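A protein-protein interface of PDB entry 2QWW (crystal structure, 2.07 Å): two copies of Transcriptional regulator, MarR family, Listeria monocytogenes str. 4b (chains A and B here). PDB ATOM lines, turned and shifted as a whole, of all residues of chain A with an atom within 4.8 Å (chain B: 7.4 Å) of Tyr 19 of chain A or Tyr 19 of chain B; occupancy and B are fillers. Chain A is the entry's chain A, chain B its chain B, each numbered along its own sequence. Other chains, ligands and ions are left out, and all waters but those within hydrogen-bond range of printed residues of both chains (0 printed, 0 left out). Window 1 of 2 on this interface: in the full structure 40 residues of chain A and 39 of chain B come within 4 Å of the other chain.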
ATOM      1  N   LEU A  15       4.093 -14.973 -18.401  1.00  0.00           N
ATOM      2  CA  LEU A  15       3.943 -14.714 -19.825  1.00  0.00           C
ATOM      3  C   LEU A  15       2.495 -14.959 -20.246  1.00  0.00           C
ATOM      4  O   LEU A  15       1.880 -14.103 -20.864  1.00  0.00           O
ATOM      5  CB  LEU A  15       4.894 -15.597 -20.644  1.00  0.00           C
ATOM      6  CG  LEU A  15       4.912 -15.370 -22.162  1.00  0.00           C
ATOM      7  CD1 LEU A  15       5.390 -13.958 -22.491  1.00  0.00           C
ATOM      8  CD2 LEU A  15       5.778 -16.419 -22.841  1.00  0.00           C
ATOM      9  N   LEU A  16       1.949 -16.106 -19.873  1.00  0.00           N
ATOM     10  CA  LEU A  16       0.582 -16.475 -20.255  1.00  0.00           C
ATOM     11  C   LEU A  16      -0.462 -15.494 -19.731  1.00  0.00           C
ATOM     12  O   LEU A  16      -1.406 -15.145 -20.455  1.00  0.00           O
ATOM     13  CB  LEU A  16       0.262 -17.924 -19.854  1.00  0.00           C
ATOM     14  CG  LEU A  16       1.098 -19.014 -20.551  1.00  0.00           C
ATOM     15  CD1 LEU A  16       0.832 -20.380 -19.950  1.00  0.00           C
ATOM     16  CD2 LEU A  16       0.875 -19.053 -22.053  1.00  0.00           C
ATOM     17  N   LYS A  17      -0.277 -15.036 -18.496  1.00  0.00           N
ATOM     18  CA  LYS A  17      -1.132 -13.999 -17.920  1.00  0.00           C
ATOM     19  C   LYS A  17      -1.016 -12.677 -18.667  1.00  0.00           C
ATOM     20  O   LYS A  17      -2.005 -11.969 -18.813  1.00  0.00           O
ATOM     21  CB  LYS A  17      -0.792 -13.734 -16.458  1.00  0.00           C
ATOM     22  CG  LYS A  17      -1.293 -14.777 -15.491  1.00  0.00           C
ATOM     23  N   THR A  18       0.187 -12.330 -19.114  1.00  0.00           N
ATOM     24  CA  THR A  18       0.394 -11.075 -19.829  1.00  0.00           C
ATOM     25  C   THR A  18      -0.250 -11.142 -21.192  1.00  0.00           C
ATOM     26  O   THR A  18      -0.940 -10.214 -21.586  1.00  0.00           O
ATOM     27  CB  THR A  18       1.878 -10.720 -19.971  1.00  0.00           C
ATOM     28  OG1 THR A  18       2.485 -10.687 -18.681  1.00  0.00           O
ATOM     29  CG2 THR A  18       2.046  -9.370 -20.595  1.00  0.00           C
ATOM     30  N   TYR A  19      -0.004 -12.219 -21.924  1.00  0.00           N
ATOM     31  CA  TYR A  19      -0.654 -12.433 -23.223  1.00  0.00           C
ATOM     32  C   TYR A  19      -2.176 -12.398 -23.111  1.00  0.00           C
ATOM     33  O   TYR A  19      -2.842 -11.810 -23.940  1.00  0.00           O
ATOM     34  CB  TYR A  19      -0.267 -13.784 -23.820  1.00  0.00           C
ATOM     35  CG  TYR A  19       1.084 -13.876 -24.488  1.00  0.00           C
ATOM     36  CD1 TYR A  19       1.603 -12.820 -25.222  1.00  0.00           C
ATOM     37  CD2 TYR A  19       1.775 -15.068 -24.502  1.00  0.00           C
ATOM     38  CE1 TYR A  19       2.821 -12.930 -25.862  1.00  0.00           C
ATOM     39  CE2 TYR A  19       2.985 -15.181 -25.145  1.00  0.00           C
ATOM     40  CZ  TYR A  19       3.506 -14.107 -25.808  1.00  0.00           C
ATOM     41  OH  TYR A  19       4.693 -14.228 -26.472  1.00  0.00           O
ATOM     42  N   TRP A  20      -2.715 -13.054 -22.084  1.00  0.00           N
ATOM     43  CA  TRP A  20      -4.148 -13.077 -21.820  1.00  0.00           C
ATOM     44  C   TRP A  20      -4.677 -11.673 -21.592  1.00  0.00           C
ATOM     45  O   TRP A  20      -5.712 -11.305 -22.112  1.00  0.00           O
ATOM     46  CB  TRP A  20      -4.447 -13.951 -20.572  1.00  0.00           C
ATOM     47  CG  TRP A  20      -5.906 -14.033 -20.267  1.00  0.00           C
ATOM     48  CD1 TRP A  20      -6.804 -14.909 -20.802  1.00  0.00           C
ATOM     49  CD2 TRP A  20      -6.654 -13.176 -19.395  1.00  0.00           C
ATOM     50  NE1 TRP A  20      -8.064 -14.650 -20.316  1.00  0.00           N
ATOM     51  CE2 TRP A  20      -8.000 -13.592 -19.452  1.00  0.00           C
ATOM     52  CE3 TRP A  20      -6.314 -12.102 -18.568  1.00  0.00           C
ATOM     53  CZ2 TRP A  20      -9.004 -12.985 -18.705  1.00  0.00           C
ATOM     54  CZ3 TRP A  20      -7.313 -11.490 -17.830  1.00  0.00           C
ATOM     55  CH2 TRP A  20      -8.643 -11.937 -17.900  1.00  0.00           C
ATOM     56  N   SER A  21      -3.956 -10.898 -20.800  1.00  0.00           N
ATOM     57  CA  SER A  21      -4.329  -9.529 -20.484  1.00  0.00           C
ATOM     58  C   SER A  21      -4.309  -8.603 -21.712  1.00  0.00           C
ATOM     59  O   SER A  21      -5.188  -7.752 -21.878  1.00  0.00           O
ATOM     60  CB  SER A  21      -3.400  -8.986 -19.426  1.00  0.00           C
ATOM     61  OG  SER A  21      -3.660  -7.619 -19.222  1.00  0.00           O
ATOM     62  N   ILE A  22      -3.304  -8.770 -22.564  1.00  0.00           N
ATOM     63  CA  ILE A  22      -3.199  -8.002 -23.817  1.00  0.00           C
ATOM     64  C   ILE A  22      -4.353  -8.363 -24.780  1.00  0.00           C
ATOM     65  O   ILE A  22      -4.836  -7.513 -25.547  1.00  0.00           O
ATOM     66  CB  ILE A  22      -1.816  -8.246 -24.510  1.00  0.00           C
ATOM     67  CG1 ILE A  22      -0.704  -7.556 -23.713  1.00  0.00           C
ATOM     68  CG2 ILE A  22      -1.820  -7.725 -25.945  1.00  0.00           C
ATOM     69  CD1 ILE A  22       0.713  -7.863 -24.186  1.00  0.00           C
ATOM     70  N   GLN A  23      -4.745  -9.630 -24.770  1.00  0.00           N
ATOM     71  CA  GLN A  23      -5.840 -10.113 -25.595  1.00  0.00           C
ATOM     72  C   GLN A  23      -7.148  -9.518 -25.065  1.00  0.00           C
ATOM     73  O   GLN A  23      -8.005  -9.150 -25.848  1.00  0.00           O
ATOM     74  CB  GLN A  23      -5.843 -11.651 -25.614  1.00  0.00           C
ATOM     75  CG  GLN A  23      -6.962 -12.362 -26.423  1.00  0.00           C
ATOM     76  CD  GLN A  23      -7.071 -11.928 -27.883  1.00  0.00           C
ATOM     77  OE1 GLN A  23      -7.430 -10.787 -28.178  1.00  0.00           O
ATOM     78  NE2 GLN A  23      -6.814 -12.859 -28.802  1.00  0.00           N
ATOM     79  N   LEU A 139      10.862  -6.915 -28.956  1.00  0.00           N
ATOM     80  CA  LEU A 139       9.473  -7.320 -28.657  1.00  0.00           C
ATOM     81  C   LEU A 139       8.919  -8.154 -29.808  1.00  0.00           C
ATOM     82  O   LEU A 139       8.406  -9.261 -29.607  1.00  0.00           O
ATOM     83  CB  LEU A 139       8.590  -6.074 -28.456  1.00  0.00           C
ATOM     84  CG  LEU A 139       7.101  -6.260 -28.158  1.00  0.00           C
ATOM     85  CD1 LEU A 139       6.847  -7.006 -26.862  1.00  0.00           C
ATOM     86  CD2 LEU A 139       6.430  -4.895 -28.122  1.00  0.00           C
ATOM     87  N   ASN A 143       8.522 -12.290 -29.636  1.00  0.00           N
ATOM     88  CA  ASN A 143       7.162 -12.810 -29.806  1.00  0.00           C
ATOM     89  C   ASN A 143       7.047 -13.702 -31.064  1.00  0.00           C
ATOM     90  O   ASN A 143       6.467 -14.797 -31.007  1.00  0.00           O
ATOM     91  CB  ASN A 143       6.124 -11.675 -29.814  1.00  0.00           C
ATOM     92  CG  ASN A 143       5.762 -11.197 -28.402  1.00  0.00           C
ATOM     93  OD1 ASN A 143       5.477 -11.994 -27.525  1.00  0.00           O
ATOM     94  ND2 ASN A 143       5.753  -9.903 -28.200  1.00  0.00           N
ATOM     95  N   VAL A 146       8.494 -16.993 -30.366  1.00  0.00           N
ATOM     96  CA  VAL A 146       7.568 -17.791 -29.579  1.00  0.00           C
ATOM     97  C   VAL A 146       6.508 -18.462 -30.473  1.00  0.00           C
ATOM     98  O   VAL A 146       6.223 -19.646 -30.317  1.00  0.00           O
ATOM     99  CB  VAL A 146       6.905 -16.970 -28.426  1.00  0.00           C
ATOM    100  CG1 VAL A 146       5.856 -17.807 -27.684  1.00  0.00           C
ATOM    101  CG2 VAL A 146       7.952 -16.493 -27.423  1.00  0.00           C
ATOM    102  N   ILE B  12       3.813  -2.577 -36.061  1.00  0.00           N
ATOM    103  CA  ILE B  12       2.567  -2.792 -35.302  1.00  0.00           C
ATOM    104  C   ILE B  12       1.781  -3.959 -35.902  1.00  0.00           C
ATOM    105  O   ILE B  12       1.322  -4.833 -35.173  1.00  0.00           O
ATOM    106  CB  ILE B  12       1.721  -1.482 -35.187  1.00  0.00           C
ATOM    107  CG1 ILE B  12       2.395  -0.502 -34.218  1.00  0.00           C
ATOM    108  CG2 ILE B  12       0.322  -1.751 -34.661  1.00  0.00           C
ATOM    109  CD1 ILE B  12       1.931   0.963 -34.386  1.00  0.00           C
ATOM    110  N   SER B  13       1.661  -3.995 -37.222  1.00  0.00           N
ATOM    111  CA  SER B  13       0.991  -5.103 -37.924  1.00  0.00           C
ATOM    112  C   SER B  13       1.596  -6.444 -37.610  1.00  0.00           C
ATOM    113  O   SER B  13       0.882  -7.400 -37.332  1.00  0.00           O
ATOM    114  CB  SER B  13       1.123  -4.935 -39.436  1.00  0.00           C
ATOM    115  OG  SER B  13       0.522  -3.740 -39.834  1.00  0.00           O
ATOM    116  N   GLU B  14       2.927  -6.507 -37.693  1.00  0.00           N
ATOM    117  CA  GLU B  14       3.679  -7.718 -37.413  1.00  0.00           C
ATOM    118  C   GLU B  14       3.438  -8.159 -35.990  1.00  0.00           C
ATOM    119  O   GLU B  14       3.250  -9.339 -35.732  1.00  0.00           O
ATOM    120  CB  GLU B  14       5.177  -7.485 -37.659  1.00  0.00           C
ATOM    121  CG  GLU B  14       5.546  -7.270 -39.113  1.00  0.00           C
ATOM    122  N   LEU B  15       3.434  -7.212 -35.059  1.00  0.00           N
ATOM    123  CA  LEU B  15       3.199  -7.537 -33.654  1.00  0.00           C
ATOM    124  C   LEU B  15       1.771  -8.033 -33.441  1.00  0.00           C
ATOM    125  O   LEU B  15       1.555  -9.026 -32.751  1.00  0.00           O
ATOM    126  CB  LEU B  15       3.495  -6.330 -32.753  1.00  0.00           C
ATOM    127  CG  LEU B  15       3.388  -6.537 -31.241  1.00  0.00           C
ATOM    128  CD1 LEU B  15       4.285  -7.681 -30.773  1.00  0.00           C
ATOM    129  CD2 LEU B  15       3.690  -5.267 -30.456  1.00  0.00           C
ATOM    130  N   LEU B  16       0.800  -7.351 -34.036  1.00  0.00           N
ATOM    131  CA  LEU B  16      -0.606  -7.730 -33.877  1.00  0.00           C
ATOM    132  C   LEU B  16      -0.897  -9.063 -34.551  1.00  0.00           C
ATOM    133  O   LEU B  16      -1.636  -9.872 -34.010  1.00  0.00           O
ATOM    134  CB  LEU B  16      -1.547  -6.630 -34.365  1.00  0.00           C
ATOM    135  CG  LEU B  16      -1.468  -5.274 -33.647  1.00  0.00           C
ATOM    136  CD1 LEU B  16      -2.606  -4.425 -34.112  1.00  0.00           C
ATOM    137  CD2 LEU B  16      -1.500  -5.397 -32.126  1.00  0.00           C
ATOM    138  N   LYS B  17      -0.291  -9.316 -35.702  1.00  0.00           N
ATOM    139  CA  LYS B  17      -0.445 -10.614 -36.351  1.00  0.00           C
ATOM    140  C   LYS B  17       0.141 -11.695 -35.454  1.00  0.00           C
ATOM    141  O   LYS B  17      -0.461 -12.742 -35.276  1.00  0.00           O
ATOM    142  CB  LYS B  17       0.240 -10.647 -37.729  1.00  0.00           C
ATOM    143  N   THR B  18       1.316 -11.423 -34.881  1.00  0.00           N
ATOM    144  CA  THR B  18       1.991 -12.379 -34.031  1.00  0.00           C
ATOM    145  C   THR B  18       1.157 -12.706 -32.800  1.00  0.00           C
ATOM    146  O   THR B  18       0.935 -13.880 -32.525  1.00  0.00           O
ATOM    147  CB  THR B  18       3.407 -11.917 -33.655  1.00  0.00           C
ATOM    148  OG1 THR B  18       4.180 -11.743 -34.846  1.00  0.00           O
ATOM    149  CG2 THR B  18       4.090 -12.946 -32.769  1.00  0.00           C
ATOM    150  N   TYR B  19       0.705 -11.693 -32.063  1.00  0.00           N
ATOM    151  CA  TYR B  19      -0.165 -11.919 -30.906  1.00  0.00           C
ATOM    152  C   TYR B  19      -1.447 -12.706 -31.295  1.00  0.00           C
ATOM    153  O   TYR B  19      -1.866 -13.629 -30.588  1.00  0.00           O
ATOM    154  CB  TYR B  19      -0.600 -10.597 -30.250  1.00  0.00           C
ATOM    155  CG  TYR B  19       0.425  -9.835 -29.429  1.00  0.00           C
ATOM    156  CD1 TYR B  19       1.293 -10.488 -28.571  1.00  0.00           C
ATOM    157  CD2 TYR B  19       0.414  -8.443 -29.395  1.00  0.00           C
ATOM    158  CE1 TYR B  19       2.179  -9.778 -27.788  1.00  0.00           C
ATOM    159  CE2 TYR B  19       1.298  -7.728 -28.608  1.00  0.00           C
ATOM    160  CZ  TYR B  19       2.166  -8.407 -27.795  1.00  0.00           C
ATOM    161  OH  TYR B  19       3.064  -7.737 -26.993  1.00  0.00           O
ATOM    162  N   TRP B  20      -2.061 -12.333 -32.413  1.00  0.00           N
ATOM    163  CA  TRP B  20      -3.252 -13.026 -32.900  1.00  0.00           C
ATOM    164  C   TRP B  20      -2.952 -14.502 -33.187  1.00  0.00           C
ATOM    165  O   TRP B  20      -3.769 -15.380 -32.909  1.00  0.00           O
ATOM    166  CB  TRP B  20      -3.791 -12.350 -34.162  1.00  0.00           C
ATOM    167  CG  TRP B  20      -5.042 -12.999 -34.706  1.00  0.00           C
ATOM    168  CD1 TRP B  20      -6.337 -12.712 -34.366  1.00  0.00           C
ATOM    169  CD2 TRP B  20      -5.110 -14.038 -35.694  1.00  0.00           C
ATOM    170  NE1 TRP B  20      -7.199 -13.513 -35.081  1.00  0.00           N
ATOM    171  CE2 TRP B  20      -6.470 -14.335 -35.898  1.00  0.00           C
ATOM    172  CE3 TRP B  20      -4.145 -14.744 -36.424  1.00  0.00           C
ATOM    173  CZ2 TRP B  20      -6.891 -15.307 -36.805  1.00  0.00           C
ATOM    174  CZ3 TRP B  20      -4.562 -15.706 -37.320  1.00  0.00           C
ATOM    175  CH2 TRP B  20      -5.925 -15.984 -37.499  1.00  0.00           C
ATOM    176  N   SER B  21      -1.774 -14.772 -33.733  1.00  0.00           N
ATOM    177  CA  SER B  21      -1.364 -16.145 -34.034  1.00  0.00           C
ATOM    178  C   SER B  21      -1.146 -16.942 -32.722  1.00  0.00           C
ATOM    179  O   SER B  21      -1.619 -18.069 -32.602  1.00  0.00           O
ATOM    180  CB  SER B  21      -0.132 -16.112 -34.932  1.00  0.00           C
ATOM    181  OG  SER B  21       0.122 -17.376 -35.488  1.00  0.00           O
ATOM    182  N   ILE B  22      -0.474 -16.344 -31.738  1.00  0.00           N
ATOM    183  CA  ILE B  22      -0.282 -16.963 -30.417  1.00  0.00           C
ATOM    184  C   ILE B  22      -1.624 -17.261 -29.747  1.00  0.00           C
ATOM    185  O   ILE B  22      -1.808 -18.351 -29.193  1.00  0.00           O
ATOM    186  CB  ILE B  22       0.597 -16.051 -29.466  1.00  0.00           C
ATOM    187  CG1 ILE B  22       2.053 -16.059 -29.943  1.00  0.00           C
ATOM    188  CG2 ILE B  22       0.546 -16.531 -28.038  1.00  0.00           C
ATOM    189  CD1 ILE B  22       2.890 -14.886 -29.473  1.00  0.00           C
ATOM    190  N   GLN B  23      -2.534 -16.285 -29.772  1.00  0.00           N
ATOM    191  CA  GLN B  23      -3.872 -16.433 -29.191  1.00  0.00           C
ATOM    192  C   GLN B  23      -4.670 -17.547 -29.888  1.00  0.00           C
ATOM    193  O   GLN B  23      -5.348 -18.322 -29.224  1.00  0.00           O
ATOM    194  CB  GLN B  23      -4.631 -15.101 -29.188  1.00  0.00           C
ATOM    195  N   ARG B  24      -4.557 -17.651 -31.209  1.00  0.00           N
ATOM    196  CA  ARG B  24      -5.187 -18.735 -31.937  1.00  0.00           C
ATOM    197  C   ARG B  24      -4.626 -20.123 -31.498  1.00  0.00           C
ATOM    198  O   ARG B  24      -5.377 -21.063 -31.303  1.00  0.00           O
ATOM    199  CB  ARG B  24      -5.011 -18.506 -33.435  1.00  0.00           C
ATOM    200  CG  ARG B  24      -5.510 -19.610 -34.339  1.00  0.00           C
ATOM    201  CD  ARG B  24      -5.442 -19.164 -35.817  1.00  0.00           C
ATOM    202  N   ILE B  25      -3.313 -20.237 -31.341  1.00  0.00           N
ATOM    203  CA  ILE B  25      -2.692 -21.479 -30.900  1.00  0.00           C
ATOM    204  C   ILE B  25      -3.125 -21.774 -29.448  1.00  0.00           C
ATOM    205  O   ILE B  25      -3.473 -22.885 -29.099  1.00  0.00           O
ATOM    206  CB  ILE B  25      -1.147 -21.411 -31.069  1.00  0.00           C
ATOM    207  CG1 ILE B  25      -0.786 -21.304 -32.567  1.00  0.00           C
ATOM    208  CG2 ILE B  25      -0.486 -22.636 -30.458  1.00  0.00           C
ATOM    209  CD1 ILE B  25       0.652 -20.830 -32.855  1.00  0.00           C
ATOM    210  N   SER B  26      -3.129 -20.755 -28.620  1.00  0.00           N
ATOM    211  CA  SER B  26      -3.557 -20.865 -27.246  1.00  0.00           C
ATOM    212  C   SER B  26      -5.018 -21.332 -27.064  1.00  0.00           C
ATOM    213  O   SER B  26      -5.336 -21.989 -26.085  1.00  0.00           O
ATOM    214  CB  SER B  26      -3.378 -19.514 -26.587  1.00  0.00           C
ATOM    215  OG  SER B  26      -2.021 -19.131 -26.710  1.00  0.00           O
ATOM    216  N   MET B 124       4.432 -24.415 -23.711  1.00  0.00           N
ATOM    217  CA  MET B 124       5.292 -23.258 -23.468  1.00  0.00           C
ATOM    218  C   MET B 124       6.631 -23.700 -22.879  1.00  0.00           C
ATOM    219  O   MET B 124       7.652 -23.089 -23.127  1.00  0.00           O
ATOM    220  CB  MET B 124       4.595 -22.248 -22.553  1.00  0.00           C
ATOM    221  CG  MET B 124       5.099 -20.822 -22.717  1.00  0.00           C
ATOM    222  SD  MET B 124       4.854 -20.148 -24.543  1.00  0.00           S
ATOM    223  CE  MET B 124       3.173 -20.459 -24.669  1.00  0.00           C
ATOM    224  N   LEU B 139      11.498 -11.267 -23.020  1.00  0.00           N
ATOM    225  CA  LEU B 139      10.138 -11.533 -23.499  1.00  0.00           C
ATOM    226  C   LEU B 139       9.110 -11.156 -22.447  1.00  0.00           C
ATOM    227  O   LEU B 139       8.125 -10.513 -22.746  1.00  0.00           O
ATOM    228  CB  LEU B 139       9.987 -13.017 -23.811  1.00  0.00           C
ATOM    229  CG  LEU B 139       8.675 -13.618 -24.311  1.00  0.00           C
ATOM    230  CD1 LEU B 139       8.262 -13.076 -25.627  1.00  0.00           C
ATOM    231  CD2 LEU B 139       8.865 -15.140 -24.412  1.00  0.00           C
ATOM    232  N   LEU B 142       9.221  -7.129 -21.788  1.00  0.00           N
ATOM    233  CA  LEU B 142       8.682  -6.307 -22.867  1.00  0.00           C
ATOM    234  C   LEU B 142       7.174  -6.430 -23.102  1.00  0.00           C
ATOM    235  O   LEU B 142       6.519  -5.434 -23.421  1.00  0.00           O
ATOM    236  CB  LEU B 142       9.465  -6.561 -24.158  1.00  0.00           C
ATOM    237  CG  LEU B 142      10.892  -6.011 -24.150  1.00  0.00           C
ATOM    238  CD1 LEU B 142      11.614  -6.413 -25.405  1.00  0.00           C
ATOM    239  CD2 LEU B 142      10.902  -4.502 -24.001  1.00  0.00           C
ATOM    240  N   ASN B 143       6.632  -7.632 -23.000  1.00  0.00           N
ATOM    241  CA  ASN B 143       5.187  -7.826 -23.090  1.00  0.00           C
ATOM    242  C   ASN B 143       4.497  -7.162 -21.899  1.00  0.00           C
ATOM    243  O   ASN B 143       3.467  -6.528 -22.078  1.00  0.00           O
ATOM    244  CB  ASN B 143       4.796  -9.310 -23.155  1.00  0.00           C
ATOM    245  CG  ASN B 143       4.996  -9.909 -24.521  1.00  0.00           C
ATOM    246  OD1 ASN B 143       4.725  -9.277 -25.541  1.00  0.00           O
ATOM    247  ND2 ASN B 143       5.452 -11.152 -24.551  1.00  0.00           N
ATOM    248  N   LYS B 144       5.044  -7.336 -20.693  1.00  0.00           N
ATOM    249  CA  LYS B 144       4.501  -6.671 -19.505  1.00  0.00           C
ATOM    250  C   LYS B 144       4.555  -5.158 -19.653  1.00  0.00           C
ATOM    251  O   LYS B 144       3.692  -4.480 -19.152  1.00  0.00           O
ATOM    252  CB  LYS B 144       5.245  -7.052 -18.226  1.00  0.00           C
ATOM    253  CG  LYS B 144       4.944  -8.407 -17.708  1.00  0.00           C
ATOM    254  CD  LYS B 144       5.748  -8.675 -16.442  1.00  0.00           C
ATOM    255  N   VAL B 146       4.278  -3.564 -22.522  1.00  0.00           N
ATOM    256  CA  VAL B 146       3.210  -3.311 -23.476  1.00  0.00           C
ATOM    257  C   VAL B 146       1.863  -3.330 -22.751  1.00  0.00           C
ATOM    258  O   VAL B 146       1.079  -2.421 -22.892  1.00  0.00           O
ATOM    259  CB  VAL B 146       3.235  -4.362 -24.627  1.00  0.00           C
ATOM    260  CG1 VAL B 146       1.962  -4.327 -25.455  1.00  0.00           C
ATOM    261  CG2 VAL B 146       4.449  -4.163 -25.511  1.00  0.00           C
ATOM    262  N   GLU B 147       1.616  -4.375 -21.970  1.00  0.00           N
ATOM    263  CA  GLU B 147       0.398  -4.493 -21.188  1.00  0.00           C
ATOM    264  C   GLU B 147       0.162  -3.256 -20.331  1.00  0.00           C
ATOM    265  O   GLU B 147      -0.919  -2.681 -20.364  1.00  0.00           O
ATOM    266  CB  GLU B 147       0.480  -5.691 -20.248  1.00  0.00           C
ATOM    267  CG  GLU B 147      -0.828  -5.993 -19.517  1.00  0.00           C
ATOM    268  CD  GLU B 147      -0.637  -6.845 -18.277  1.00  0.00           C
ATOM    269  OE1 GLU B 147       0.515  -7.224 -17.973  1.00  0.00           O
ATOM    270  OE2 GLU B 147      -1.643  -7.138 -17.598  1.00  0.00           O
ATOM    271  N   LEU B 150      -0.564  -0.162 -22.259  1.00  0.00           N
ATOM    272  CA  LEU B 150      -1.916  -0.245 -22.801  1.00  0.00           C
ATOM    273  C   LEU B 150      -2.937   0.107 -21.735  1.00  0.00           C
ATOM    274  O   LEU B 150      -3.906   0.800 -22.024  1.00  0.00           O
ATOM    275  CB  LEU B 150      -2.227  -1.632 -23.365  1.00  0.00           C
ATOM    276  CG  LEU B 150      -1.690  -2.024 -24.745  1.00  0.00           C
ATOM    277  CD1 LEU B 150      -2.017  -3.466 -25.023  1.00  0.00           C
ATOM    278  CD2 LEU B 150      -2.272  -1.175 -25.845  1.00  0.00           C
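OE2 of Glu 147 of chain B is in hydrogen-bond range of OG of Ser 21 of chain A, at 2.6 Å. The side-chain amide oxygen (OD1) of Asn 143 of chain B is in hydrogen-bond range of the side-chain amide nitrogen (ND2) of Asn 143 of chain A (2.9 Å).
OD1 of Asn 143 of chain A sits at hydrogen-bond distance from OH of Tyr 19 of chain A, at 2.6 Å. O of Leu 139 of chain A sits at hydrogen-bond distance from ND2 of Asn 143 of chain A, at 3.1 Å. O of Glu 14 of chain B is in hydrogen-bond range of OG1 of Thr 18 of chain B. OD1 of Asn 143 of chain B is in hydrogen-bond range of OH of Tyr 19 of chain B (2.7 Å). The backbone carbonyl oxygen (O) of Ile 22 of chain B sits at hydrogen-bond distance from the side-chain hydroxyl (OG) of Ser 26 of chain B (2.6 Å). The backbone carbonyl oxygen (O) of Leu 139 of chain B is in hydrogen-bond range of the side-chain amide nitrogen (ND2) of Asn 143 of chain B, 3.3 Å away.
Among the printed residues, pairs that only touch across the chains: Gln 23 of chain A with Gln 23 of chain B, Leu 139 of chain A with Val 146 of chain B, Leu 139 of chain A with Asn 143 of chain B, Val 146 of chain A with Leu 139 of chain B, Tyr 19 of chain A with Asn 143 of chain B, Leu 15 of chain A with Asn 143 of chain B, Asn 143 of chain A with Thr 18 of chain B, Thr 18 of chain A with Lys 144 of chain B, Thr 18 of chain A with Asn 143 of chain B, Asn 143 of chain A with Leu 139 of chain B, Tyr 19 of chain A with Ile 22 of chain B, Asn 143 of chain A with Tyr 19 of chain B, Leu 139 of chain A with Leu 15 of chain B, Ile 22 of chain A with Tyr 19 of chain B, Leu 139 of chain A with Leu 142 of chain B, Leu 15 of chain A with Leu 139 of chain B, Asn 143 of chain A with Leu 15 of chain B, Ile 22 of chain A with Asn 143 of chain B, Thr 18 of chain A with Glu 147 of chain B, Tyr 19 of chain A with Tyr 19 of chain B, Leu 16 of chain A with Met 124 of chain B, Tyr 19 of chain A with Leu 139 of chain B, Leu 139 of chain A with Tyr 19 of chain B, Asn 143 of chain A with Ile 22 of chain B and Ile 22 of chain A with Val 146 of chain B.
Tyr 19 of chain A touches just these residues of chain B: Tyr 19 (3.7 Å), Ile 22 (3.6 Å), Leu 139 (3.8 Å) and Asn 143 (3.4 Å). Printed residues of chain B within 4 Å of Ser 21 of chain A: Glu 147 (2.6 Å). Ser 13 of chain B touches none of the printed residues of chain A. Leu 16 of chain B touches none of the printed residues of chain A. Tyr 19 of chain B touches just these residues of chain A: Tyr 19, Ile 22, Leu 139 and Asn 143. Printed residues of chain A within 4 Å of Gln 23 of chain B: Gln 23 (3.2 Å). Of the printed residues of chain A, Leu 139 of chain B touches Leu 15 (3.7 Å), Tyr 19 (3.8 Å), Asn 143 (3.5 Å) and Val 146 (3.4 Å).
Of the 23 printed residues of chain B, 12 touch a printed residue of chain A. Hydrophobic or aromatic side chains of chain B within 4 Å of the printed part of chain A: Leu 15, Tyr 19, Ile 22, Met 124, Leu 139, Leu 142 and Val 146. Of the 12 printed residues of chain A, 10 touch a printed residue of chain B. Among the printed residues, no Asp or Glu carboxylate lies within 4 Å of a Lys or Arg side-chain nitrogen of the other chain.
Leu 15 of chain A touches Asn 143 of chain B, and with the chains exchanged Asn 143 of chain A touches Leu 15 of chain B. Tyr 19 of chain A touches Ile 22 of chain B, and with the chains exchanged Ile 22 of chain A touches Tyr 19 of chain B. Ile 22 of chain A touches Asn 143 of chain B, and with the chains exchanged Asn 143 of chain A touches Ile 22 of chain B. Leu 139 of chain A touches Val 146 of chain B, and with the chains exchanged Val 146 of chain A touches Leu 139 of chain B. Of the 27 pairs that touch across the chains among the printed residues, 21 have their exchanged pair printed and touching as well.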
